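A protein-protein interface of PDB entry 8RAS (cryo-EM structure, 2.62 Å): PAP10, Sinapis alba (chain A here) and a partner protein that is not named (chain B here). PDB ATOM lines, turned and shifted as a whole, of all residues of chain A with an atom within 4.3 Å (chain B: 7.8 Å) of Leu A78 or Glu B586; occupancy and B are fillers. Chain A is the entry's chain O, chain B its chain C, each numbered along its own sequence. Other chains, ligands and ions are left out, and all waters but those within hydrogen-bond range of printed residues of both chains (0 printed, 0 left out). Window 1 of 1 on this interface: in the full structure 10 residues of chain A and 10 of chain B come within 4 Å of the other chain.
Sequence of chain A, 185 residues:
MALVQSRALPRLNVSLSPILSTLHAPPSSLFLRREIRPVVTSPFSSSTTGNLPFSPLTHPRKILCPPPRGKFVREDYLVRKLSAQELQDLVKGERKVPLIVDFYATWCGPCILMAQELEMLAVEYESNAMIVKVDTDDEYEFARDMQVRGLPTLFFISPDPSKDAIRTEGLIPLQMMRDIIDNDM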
ATOM      1  N   ARG A  74      -9.774 -28.399 -26.277  1.00  0.00           N
ATOM      2  CA  ARG A  74      -8.559 -27.785 -25.760  1.00  0.00           C
ATOM      3  C   ARG A  74      -8.507 -26.310 -26.140  1.00  0.00           C
ATOM      4  O   ARG A  74      -8.987 -25.900 -27.199  1.00  0.00           O
ATOM      5  CB  ARG A  74      -7.333 -28.514 -26.312  1.00  0.00           C
ATOM      6  CG  ARG A  74      -6.013 -28.193 -25.631  1.00  0.00           C
ATOM      7  CD  ARG A  74      -6.057 -28.473 -24.140  1.00  0.00           C
ATOM      8  NE  ARG A  74      -4.716 -28.539 -23.572  1.00  0.00           N
ATOM      9  CZ  ARG A  74      -4.270 -27.750 -22.605  1.00  0.00           C
ATOM     10  NH1 ARG A  74      -5.038 -26.825 -22.058  1.00  0.00           N
ATOM     11  NH2 ARG A  74      -3.021 -27.898 -22.172  1.00  0.00           N
ATOM     12  N   TYR A  77      -4.563 -21.301 -26.847  1.00  0.00           N
ATOM     13  CA  TYR A  77      -3.455 -20.479 -26.382  1.00  0.00           C
ATOM     14  C   TYR A  77      -3.088 -20.873 -24.961  1.00  0.00           C
ATOM     15  O   TYR A  77      -3.964 -20.989 -24.098  1.00  0.00           O
ATOM     16  CB  TYR A  77      -3.810 -18.991 -26.455  1.00  0.00           C
ATOM     17  CG  TYR A  77      -4.302 -18.572 -27.819  1.00  0.00           C
ATOM     18  CD1 TYR A  77      -3.410 -18.230 -28.824  1.00  0.00           C
ATOM     19  CD2 TYR A  77      -5.659 -18.537 -28.106  1.00  0.00           C
ATOM     20  CE1 TYR A  77      -3.856 -17.856 -30.075  1.00  0.00           C
ATOM     21  CE2 TYR A  77      -6.113 -18.164 -29.353  1.00  0.00           C
ATOM     22  CZ  TYR A  77      -5.208 -17.825 -30.333  1.00  0.00           C
ATOM     23  OH  TYR A  77      -5.660 -17.451 -31.576  1.00  0.00           O
ATOM     24  N   LEU A  78      -1.792 -21.075 -24.721  1.00  0.00           N
ATOM     25  CA  LEU A  78      -1.299 -21.476 -23.412  1.00  0.00           C
ATOM     26  C   LEU A  78      -0.713 -20.326 -22.608  1.00  0.00           C
ATOM     27  O   LEU A  78      -0.570 -20.456 -21.388  1.00  0.00           O
ATOM     28  CB  LEU A  78      -0.236 -22.571 -23.558  1.00  0.00           C
ATOM     29  CG  LEU A  78      -0.675 -23.867 -24.238  1.00  0.00           C
ATOM     30  CD1 LEU A  78       0.470 -24.861 -24.263  1.00  0.00           C
ATOM     31  CD2 LEU A  78      -1.886 -24.455 -23.538  1.00  0.00           C
ATOM     32  N   VAL A  79      -0.369 -19.216 -23.252  1.00  0.00           N
ATOM     33  CA  VAL A  79       0.190 -18.068 -22.549  1.00  0.00           C
ATOM     34  C   VAL A  79      -0.949 -17.247 -21.964  1.00  0.00           C
ATOM     35  O   VAL A  79      -1.867 -16.833 -22.680  1.00  0.00           O
ATOM     36  CB  VAL A  79       1.062 -17.225 -23.492  1.00  0.00           C
ATOM     37  CG1 VAL A  79       1.584 -15.992 -22.775  1.00  0.00           C
ATOM     38  CG2 VAL A  79       2.212 -18.058 -24.030  1.00  0.00           C
ATOM     39  N   ARG A  80      -0.893 -17.012 -20.657  1.00  0.00           N
ATOM     40  CA  ARG A  80      -1.954 -16.328 -19.935  1.00  0.00           C
ATOM     41  C   ARG A  80      -1.620 -14.853 -19.769  1.00  0.00           C
ATOM     42  O   ARG A  80      -0.462 -14.487 -19.550  1.00  0.00           O
ATOM     43  CB  ARG A  80      -2.178 -16.969 -18.564  1.00  0.00           C
ATOM     44  CG  ARG A  80      -3.608 -17.410 -18.318  1.00  0.00           C
ATOM     45  CD  ARG A  80      -4.056 -18.419 -19.360  1.00  0.00           C
ATOM     46  NE  ARG A  80      -3.305 -19.666 -19.269  1.00  0.00           N
ATOM     47  CZ  ARG A  80      -3.589 -20.762 -19.959  1.00  0.00           C
ATOM     48  NH1 ARG A  80      -4.605 -20.803 -20.804  1.00  0.00           N
ATOM     49  NH2 ARG A  80      -2.833 -21.844 -19.795  1.00  0.00           N
ATOM     50  N   GLU A 119       4.124 -18.824 -27.820  1.00  0.00           N
ATOM     51  CA  GLU A 119       3.245 -19.989 -27.806  1.00  0.00           C
ATOM     52  C   GLU A 119       4.037 -21.270 -28.041  1.00  0.00           C
ATOM     53  O   GLU A 119       3.828 -22.279 -27.353  1.00  0.00           O
ATOM     54  CB  GLU A 119       2.147 -19.831 -28.856  1.00  0.00           C
ATOM     55  CG  GLU A 119       1.020 -18.912 -28.432  1.00  0.00           C
ATOM     56  CD  GLU A 119       0.164 -19.509 -27.336  1.00  0.00           C
ATOM     57  OE1 GLU A 119       0.066 -20.753 -27.268  1.00  0.00           O
ATOM     58  OE2 GLU A 119      -0.407 -18.737 -26.542  1.00  0.00           O
ATOM     59  N   ALA A 122       5.964 -22.011 -24.866  1.00  0.00           N
ATOM     60  CA  ALA A 122       5.087 -22.562 -23.840  1.00  0.00           C
ATOM     61  C   ALA A 122       4.769 -24.022 -24.119  1.00  0.00           C
ATOM     62  O   ALA A 122       4.685 -24.835 -23.192  1.00  0.00           O
ATOM     63  CB  ALA A 122       3.801 -21.740 -23.749  1.00  0.00           C
ATOM     64  N   VAL A 123       4.574 -24.374 -25.391  1.00  0.00           N
ATOM     65  CA  VAL A 123       4.396 -25.781 -25.741  1.00  0.00           C
ATOM     66  C   VAL A 123       5.647 -26.577 -25.388  1.00  0.00           C
ATOM     67  O   VAL A 123       5.565 -27.714 -24.907  1.00  0.00           O
ATOM     68  CB  VAL A 123       4.031 -25.926 -27.229  1.00  0.00           C
ATOM     69  CG1 VAL A 123       4.041 -27.387 -27.639  1.00  0.00           C
ATOM     70  CG2 VAL A 123       2.671 -25.310 -27.502  1.00  0.00           C
ATOM     71  N   ALA B 583      -3.595 -31.496 -35.628  1.00  0.00           N
ATOM     72  CA  ALA B 583      -3.508 -31.799 -34.207  1.00  0.00           C
ATOM     73  C   ALA B 583      -4.680 -31.196 -33.443  1.00  0.00           C
ATOM     74  O   ALA B 583      -5.061 -30.043 -33.663  1.00  0.00           O
ATOM     75  CB  ALA B 583      -2.191 -31.280 -33.633  1.00  0.00           C
ATOM     76  N   GLU B 584      -5.253 -31.988 -32.541  1.00  0.00           N
ATOM     77  CA  GLU B 584      -6.319 -31.532 -31.661  1.00  0.00           C
ATOM     78  C   GLU B 584      -5.820 -31.198 -30.263  1.00  0.00           C
ATOM     79  O   GLU B 584      -6.628 -30.866 -29.392  1.00  0.00           O
ATOM     80  CB  GLU B 584      -7.422 -32.591 -31.574  1.00  0.00           C
ATOM     81  CG  GLU B 584      -7.666 -33.337 -32.873  1.00  0.00           C
ATOM     82  CD  GLU B 584      -9.080 -33.871 -32.983  1.00  0.00           C
ATOM     83  OE1 GLU B 584     -10.023 -33.055 -33.039  1.00  0.00           O
ATOM     84  OE2 GLU B 584      -9.248 -35.108 -33.017  1.00  0.00           O
ATOM     85  N   HIS B 585      -4.512 -31.276 -30.033  1.00  0.00           N
ATOM     86  CA  HIS B 585      -3.934 -31.046 -28.719  1.00  0.00           C
ATOM     87  C   HIS B 585      -2.454 -30.747 -28.894  1.00  0.00           C
ATOM     88  O   HIS B 585      -1.782 -31.390 -29.703  1.00  0.00           O
ATOM     89  CB  HIS B 585      -4.133 -32.264 -27.810  1.00  0.00           C
ATOM     90  CG  HIS B 585      -4.051 -31.952 -26.348  1.00  0.00           C
ATOM     91  ND1 HIS B 585      -2.859 -31.702 -25.706  1.00  0.00           N
ATOM     92  CD2 HIS B 585      -5.016 -31.856 -25.402  1.00  0.00           C
ATOM     93  CE1 HIS B 585      -3.091 -31.462 -24.428  1.00  0.00           C
ATOM     94  NE2 HIS B 585      -4.392 -31.550 -24.218  1.00  0.00           N
ATOM     95  N   GLU B 586      -1.954 -29.771 -28.143  1.00  0.00           N
ATOM     96  CA  GLU B 586      -0.535 -29.462 -28.191  1.00  0.00           C
ATOM     97  C   GLU B 586       0.263 -30.548 -27.479  1.00  0.00           C
ATOM     98  O   GLU B 586      -0.246 -31.253 -26.605  1.00  0.00           O
ATOM     99  CB  GLU B 586      -0.257 -28.099 -27.557  1.00  0.00           C
ATOM    100  CG  GLU B 586      -0.130 -28.122 -26.043  1.00  0.00           C
ATOM    101  CD  GLU B 586      -1.464 -27.962 -25.345  1.00  0.00           C
ATOM    102  OE1 GLU B 586      -2.457 -27.633 -26.026  1.00  0.00           O
ATOM    103  OE2 GLU B 586      -1.521 -28.167 -24.116  1.00  0.00           O
ATOM    104  N   GLY B 587       1.521 -30.689 -27.870  1.00  0.00           N
ATOM    105  CA  GLY B 587       2.358 -31.700 -27.245  1.00  0.00           C
ATOM    106  C   GLY B 587       3.601 -31.970 -28.076  1.00  0.00           C
ATOM    107  O   GLY B 587       4.076 -31.099 -28.805  1.00  0.00           O
ATOM    108  N   LYS B 588       4.108 -33.193 -27.938  1.00  0.00           N
ATOM    109  CA  LYS B 588       5.326 -33.624 -28.605  1.00  0.00           C
ATOM    110  C   LYS B 588       5.058 -34.901 -29.385  1.00  0.00           C
ATOM    111  O   LYS B 588       4.193 -35.703 -29.019  1.00  0.00           O
ATOM    112  CB  LYS B 588       6.460 -33.867 -27.601  1.00  0.00           C
ATOM    113  CG  LYS B 588       6.367 -33.027 -26.338  1.00  0.00           C
ATOM    114  CD  LYS B 588       7.201 -31.768 -26.452  1.00  0.00           C
ATOM    115  CE  LYS B 588       7.671 -31.286 -25.089  1.00  0.00           C
ATOM    116  NZ  LYS B 588       9.082 -31.674 -24.820  1.00  0.00           N
ATOM    117  N   ILE B 589       5.808 -35.084 -30.465  1.00  0.00           N
ATOM    118  CA  ILE B 589       5.714 -36.285 -31.285  1.00  0.00           C
ATOM    119  C   ILE B 589       6.655 -37.338 -30.719  1.00  0.00           C
ATOM    120  O   ILE B 589       7.841 -37.070 -30.497  1.00  0.00           O
ATOM    121  CB  ILE B 589       6.048 -35.978 -32.753  1.00  0.00           C
ATOM    122  CG1 ILE B 589       5.092 -34.920 -33.305  1.00  0.00           C
ATOM    123  CG2 ILE B 589       5.985 -37.246 -33.588  1.00  0.00           C
ATOM    124  CD1 ILE B 589       3.667 -35.403 -33.433  1.00  0.00           C
ATOM    125  N   LEU B 599       0.879 -38.837 -30.496  1.00  0.00           N
ATOM    126  CA  LEU B 599       1.124 -37.501 -29.970  1.00  0.00           C
ATOM    127  C   LEU B 599       0.779 -37.483 -28.489  1.00  0.00           C
ATOM    128  O   LEU B 599      -0.271 -37.995 -28.087  1.00  0.00           O
ATOM    129  CB  LEU B 599       0.303 -36.452 -30.724  1.00  0.00           C
ATOM    130  CG  LEU B 599       0.556 -34.988 -30.356  1.00  0.00           C
ATOM    131  CD1 LEU B 599       0.702 -34.144 -31.608  1.00  0.00           C
ATOM    132  CD2 LEU B 599      -0.563 -34.452 -29.478  1.00  0.00           C
ATOM    133  N   SER B 600       1.660 -36.897 -27.683  1.00  0.00           N
ATOM    134  CA  SER B 600       1.470 -36.817 -26.240  1.00  0.00           C
ATOM    135  C   SER B 600       1.701 -35.388 -25.778  1.00  0.00           C
ATOM    136  O   SER B 600       2.724 -34.782 -26.112  1.00  0.00           O
ATOM    137  CB  SER B 600       2.418 -37.766 -25.503  1.00  0.00           C
ATOM    138  OG  SER B 600       3.646 -37.124 -25.204  1.00  0.00           O
ATOM    139  N   GLY B 601       0.757 -34.859 -25.005  1.00  0.00           N
ATOM    140  CA  GLY B 601       0.887 -33.521 -24.465  1.00  0.00           C
ATOM    141  C   GLY B 601      -0.003 -33.275 -23.265  1.00  0.00           C
ATOM    142  O   GLY B 601      -1.186 -33.631 -23.282  1.00  0.00           O
ATOM    143  N   ASN B 602       0.558 -32.661 -22.221  1.00  0.00           N
ATOM    144  CA  ASN B 602      -0.172 -32.350 -20.990  1.00  0.00           C
ATOM    145  C   ASN B 602      -0.815 -33.603 -20.396  1.00  0.00           C
ATOM    146  O   ASN B 602      -2.016 -33.646 -20.123  1.00  0.00           O
ATOM    147  CB  ASN B 602      -1.217 -31.258 -21.232  1.00  0.00           C
ATOM    148  CG  ASN B 602      -1.623 -30.549 -19.956  1.00  0.00           C
ATOM    149  OD1 ASN B 602      -0.797 -30.310 -19.076  1.00  0.00           O
ATOM    150  ND2 ASN B 602      -2.903 -30.212 -19.847  1.00  0.00           N
ATOM    151  N   GLU B 603       0.007 -34.637 -20.204  1.00  0.00           N
ATOM    152  CA  GLU B 603      -0.413 -35.920 -19.644  1.00  0.00           C
ATOM    153  C   GLU B 603      -1.533 -36.572 -20.451  1.00  0.00           C
ATOM    154  O   GLU B 603      -2.279 -37.402 -19.923  1.00  0.00           O
ATOM    155  CB  GLU B 603      -0.838 -35.777 -18.176  1.00  0.00           C
ATOM    156  CG  GLU B 603       0.068 -34.883 -17.344  1.00  0.00           C
ATOM    157  CD  GLU B 603       1.508 -35.355 -17.340  1.00  0.00           C
ATOM    158  OE1 GLU B 603       1.744 -36.548 -17.056  1.00  0.00           O
ATOM    159  OE2 GLU B 603       2.406 -34.533 -17.621  1.00  0.00           O
ATOM    160  N   ASN B 604      -1.664 -36.213 -21.727  1.00  0.00           N
ATOM    161  CA  ASN B 604      -2.688 -36.768 -22.605  1.00  0.00           C
ATOM    162  C   ASN B 604      -2.001 -37.329 -23.842  1.00  0.00           C
ATOM    163  O   ASN B 604      -1.444 -36.571 -24.643  1.00  0.00           O
ATOM    164  CB  ASN B 604      -3.723 -35.708 -22.989  1.00  0.00           C
ATOM    165  CG  ASN B 604      -4.771 -35.499 -21.914  1.00  0.00           C
ATOM    166  OD1 ASN B 604      -4.555 -35.826 -20.747  1.00  0.00           O
ATOM    167  ND2 ASN B 604      -5.917 -34.953 -22.304  1.00  0.00           N
ATOM    168  N   LEU B 606      -2.486 -39.454 -27.311  1.00  0.00           N
ATOM    169  CA  LEU B 606      -3.482 -39.846 -28.295  1.00  0.00           C
ATOM    170  C   LEU B 606      -2.823 -40.627 -29.422  1.00  0.00           C
ATOM    171  O   LEU B 606      -1.638 -40.446 -29.718  1.00  0.00           O
ATOM    172  CB  LEU B 606      -4.211 -38.625 -28.870  1.00  0.00           C
ATOM    173  CG  LEU B 606      -4.400 -37.419 -27.946  1.00  0.00           C
ATOM    174  CD1 LEU B 606      -4.985 -36.246 -28.714  1.00  0.00           C
ATOM    175  CD2 LEU B 606      -5.286 -37.776 -26.762  1.00  0.00           C
ATOM    176  N   CYS B 633       7.856 -30.441 -31.343  1.00  0.00           N
ATOM    177  CA  CYS B 633       6.778 -29.797 -30.608  1.00  0.00           C
ATOM    178  C   CYS B 633       5.683 -29.341 -31.561  1.00  0.00           C
ATOM    179  O   CYS B 633       5.958 -28.846 -32.658  1.00  0.00           O
ATOM    180  CB  CYS B 633       7.311 -28.609 -29.814  1.00  0.00           C
ATOM    181  SG  CYS B 633       8.275 -29.086 -28.375  1.00  0.00           S
ATOM    182  N   ILE B 634       4.434 -29.508 -31.134  1.00  0.00           N
ATOM    183  CA  ILE B 634       3.271 -29.283 -31.982  1.00  0.00           C
ATOM    184  C   ILE B 634       2.288 -28.385 -31.245  1.00  0.00           C
ATOM    185  O   ILE B 634       2.010 -28.602 -30.061  1.00  0.00           O
ATOM    186  CB  ILE B 634       2.599 -30.614 -32.374  1.00  0.00           C
ATOM    187  CG1 ILE B 634       3.560 -31.476 -33.194  1.00  0.00           C
ATOM    188  CG2 ILE B 634       1.323 -30.366 -33.152  1.00  0.00           C
ATOM    189  CD1 ILE B 634       3.726 -31.014 -34.622  1.00  0.00           C
ATOM    190  N   LYS B 635       1.774 -27.375 -31.940  1.00  0.00           N
ATOM    191  CA  LYS B 635       0.673 -26.567 -31.438  1.00  0.00           C
ATOM    192  C   LYS B 635      -0.653 -27.202 -31.829  1.00  0.00           C
ATOM    193  O   LYS B 635      -0.741 -27.939 -32.814  1.00  0.00           O
ATOM    194  CB  LYS B 635       0.733 -25.145 -31.994  1.00  0.00           C
ATOM    195  CG  LYS B 635       1.888 -24.303 -31.502  1.00  0.00           C
ATOM    196  CD  LYS B 635       1.751 -22.884 -32.023  1.00  0.00           C
ATOM    197  CE  LYS B 635       3.042 -22.108 -31.897  1.00  0.00           C
ATOM    198  NZ  LYS B 635       2.922 -20.764 -32.522  1.00  0.00           N
ATOM    199  N   LYS B 636      -1.691 -26.908 -31.052  1.00  0.00           N
ATOM    200  CA  LYS B 636      -3.024 -27.372 -31.406  1.00  0.00           C
ATOM    201  C   LYS B 636      -3.478 -26.695 -32.692  1.00  0.00           C
ATOM    202  O   LYS B 636      -3.478 -25.465 -32.792  1.00  0.00           O
ATOM    203  CB  LYS B 636      -4.015 -27.087 -30.281  1.00  0.00           C
ATOM    204  CG  LYS B 636      -5.464 -27.107 -30.731  1.00  0.00           C
ATOM    205  CD  LYS B 636      -6.415 -27.008 -29.560  1.00  0.00           C
ATOM    206  CE  LYS B 636      -7.854 -26.918 -30.030  1.00  0.00           C
ATOM    207  NZ  LYS B 636      -8.152 -27.911 -31.093  1.00  0.00           N
ATOM    208  N   GLY B 637      -3.867 -27.499 -33.677  1.00  0.00           N
ATOM    209  CA  GLY B 637      -4.283 -26.990 -34.965  1.00  0.00           C
ATOM    210  C   GLY B 637      -3.215 -27.002 -36.035  1.00  0.00           C
ATOM    211  O   GLY B 637      -3.463 -26.497 -37.135  1.00  0.00           O
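Among the printed residues, Asp or Glu carboxylates within 4 Å of a Lys or Arg side-chain nitrogen of the other chain: Arg A74 with Glu B586 (2.5 Å).
Leu A78 touches just one residue of chain B: Glu B586 (3.8 Å). Glu B586 touches just these residues of chain A: Arg A74 and Leu A78. Printed residues of chain A within 4 Å of Asn B602: Arg A74 (3.3 Å). Of the printed residues of chain B, Glu A119 touches Lys B635 (3.9 Å). Of the printed residues of chain A, Ile B634 touches Val A123. Cys B633 touches none of the printed residues of chain A. Gly B601 touches none of the printed residues of chain A. The nearest residue of chain A that does not touch Glu B586 is Val A123 (4.04 Å).
O of Leu A78 lies within hydrogen-bond range of NH2 of Arg A80 (3.1 Å). The backbone NH (N) of Leu A78 lies within hydrogen-bond range of the side-chain carboxylate (OE1) of Glu A119, at 3.2 Å. N of Val A79 sits at hydrogen-bond distance from OE2 of Glu A119 (3.3 Å). N of Ile B634 sits at hydrogen-bond distance from O of Gly B587, 2.8 Å away. The backbone carbonyl oxygen (O) of Asn B602 lies close to the side-chain amide oxygen (OD1) of Asn B604, 3.4 Å away.
Glu B584 touches Arg A74 (O to CB, 3.9 Å). Arg A74 touches Lys B636. Leu A78 touches Glu B586 (CD1 to CG, 3.8 Å). Glu A119 touches Lys B635. O of Gly B587 touches CG1 of Val A123, 3.9 Å away. CG1 of Val A123 touches O of Ile B634, 3.4 Å away.
A ring nitrogen (NE2) of His B585 sits at hydrogen-bond distance from the guanidinium group (NE) of Arg A74, 3.1 Å away. NH2 of Arg A74 is in salt-bridge range of OE2 of Glu B586, 2.5 Å away. The guanidinium group (NH2) of Arg A74 sits close to the side-chain amide nitrogen (ND2) of Asn B602 (3.3 Å).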
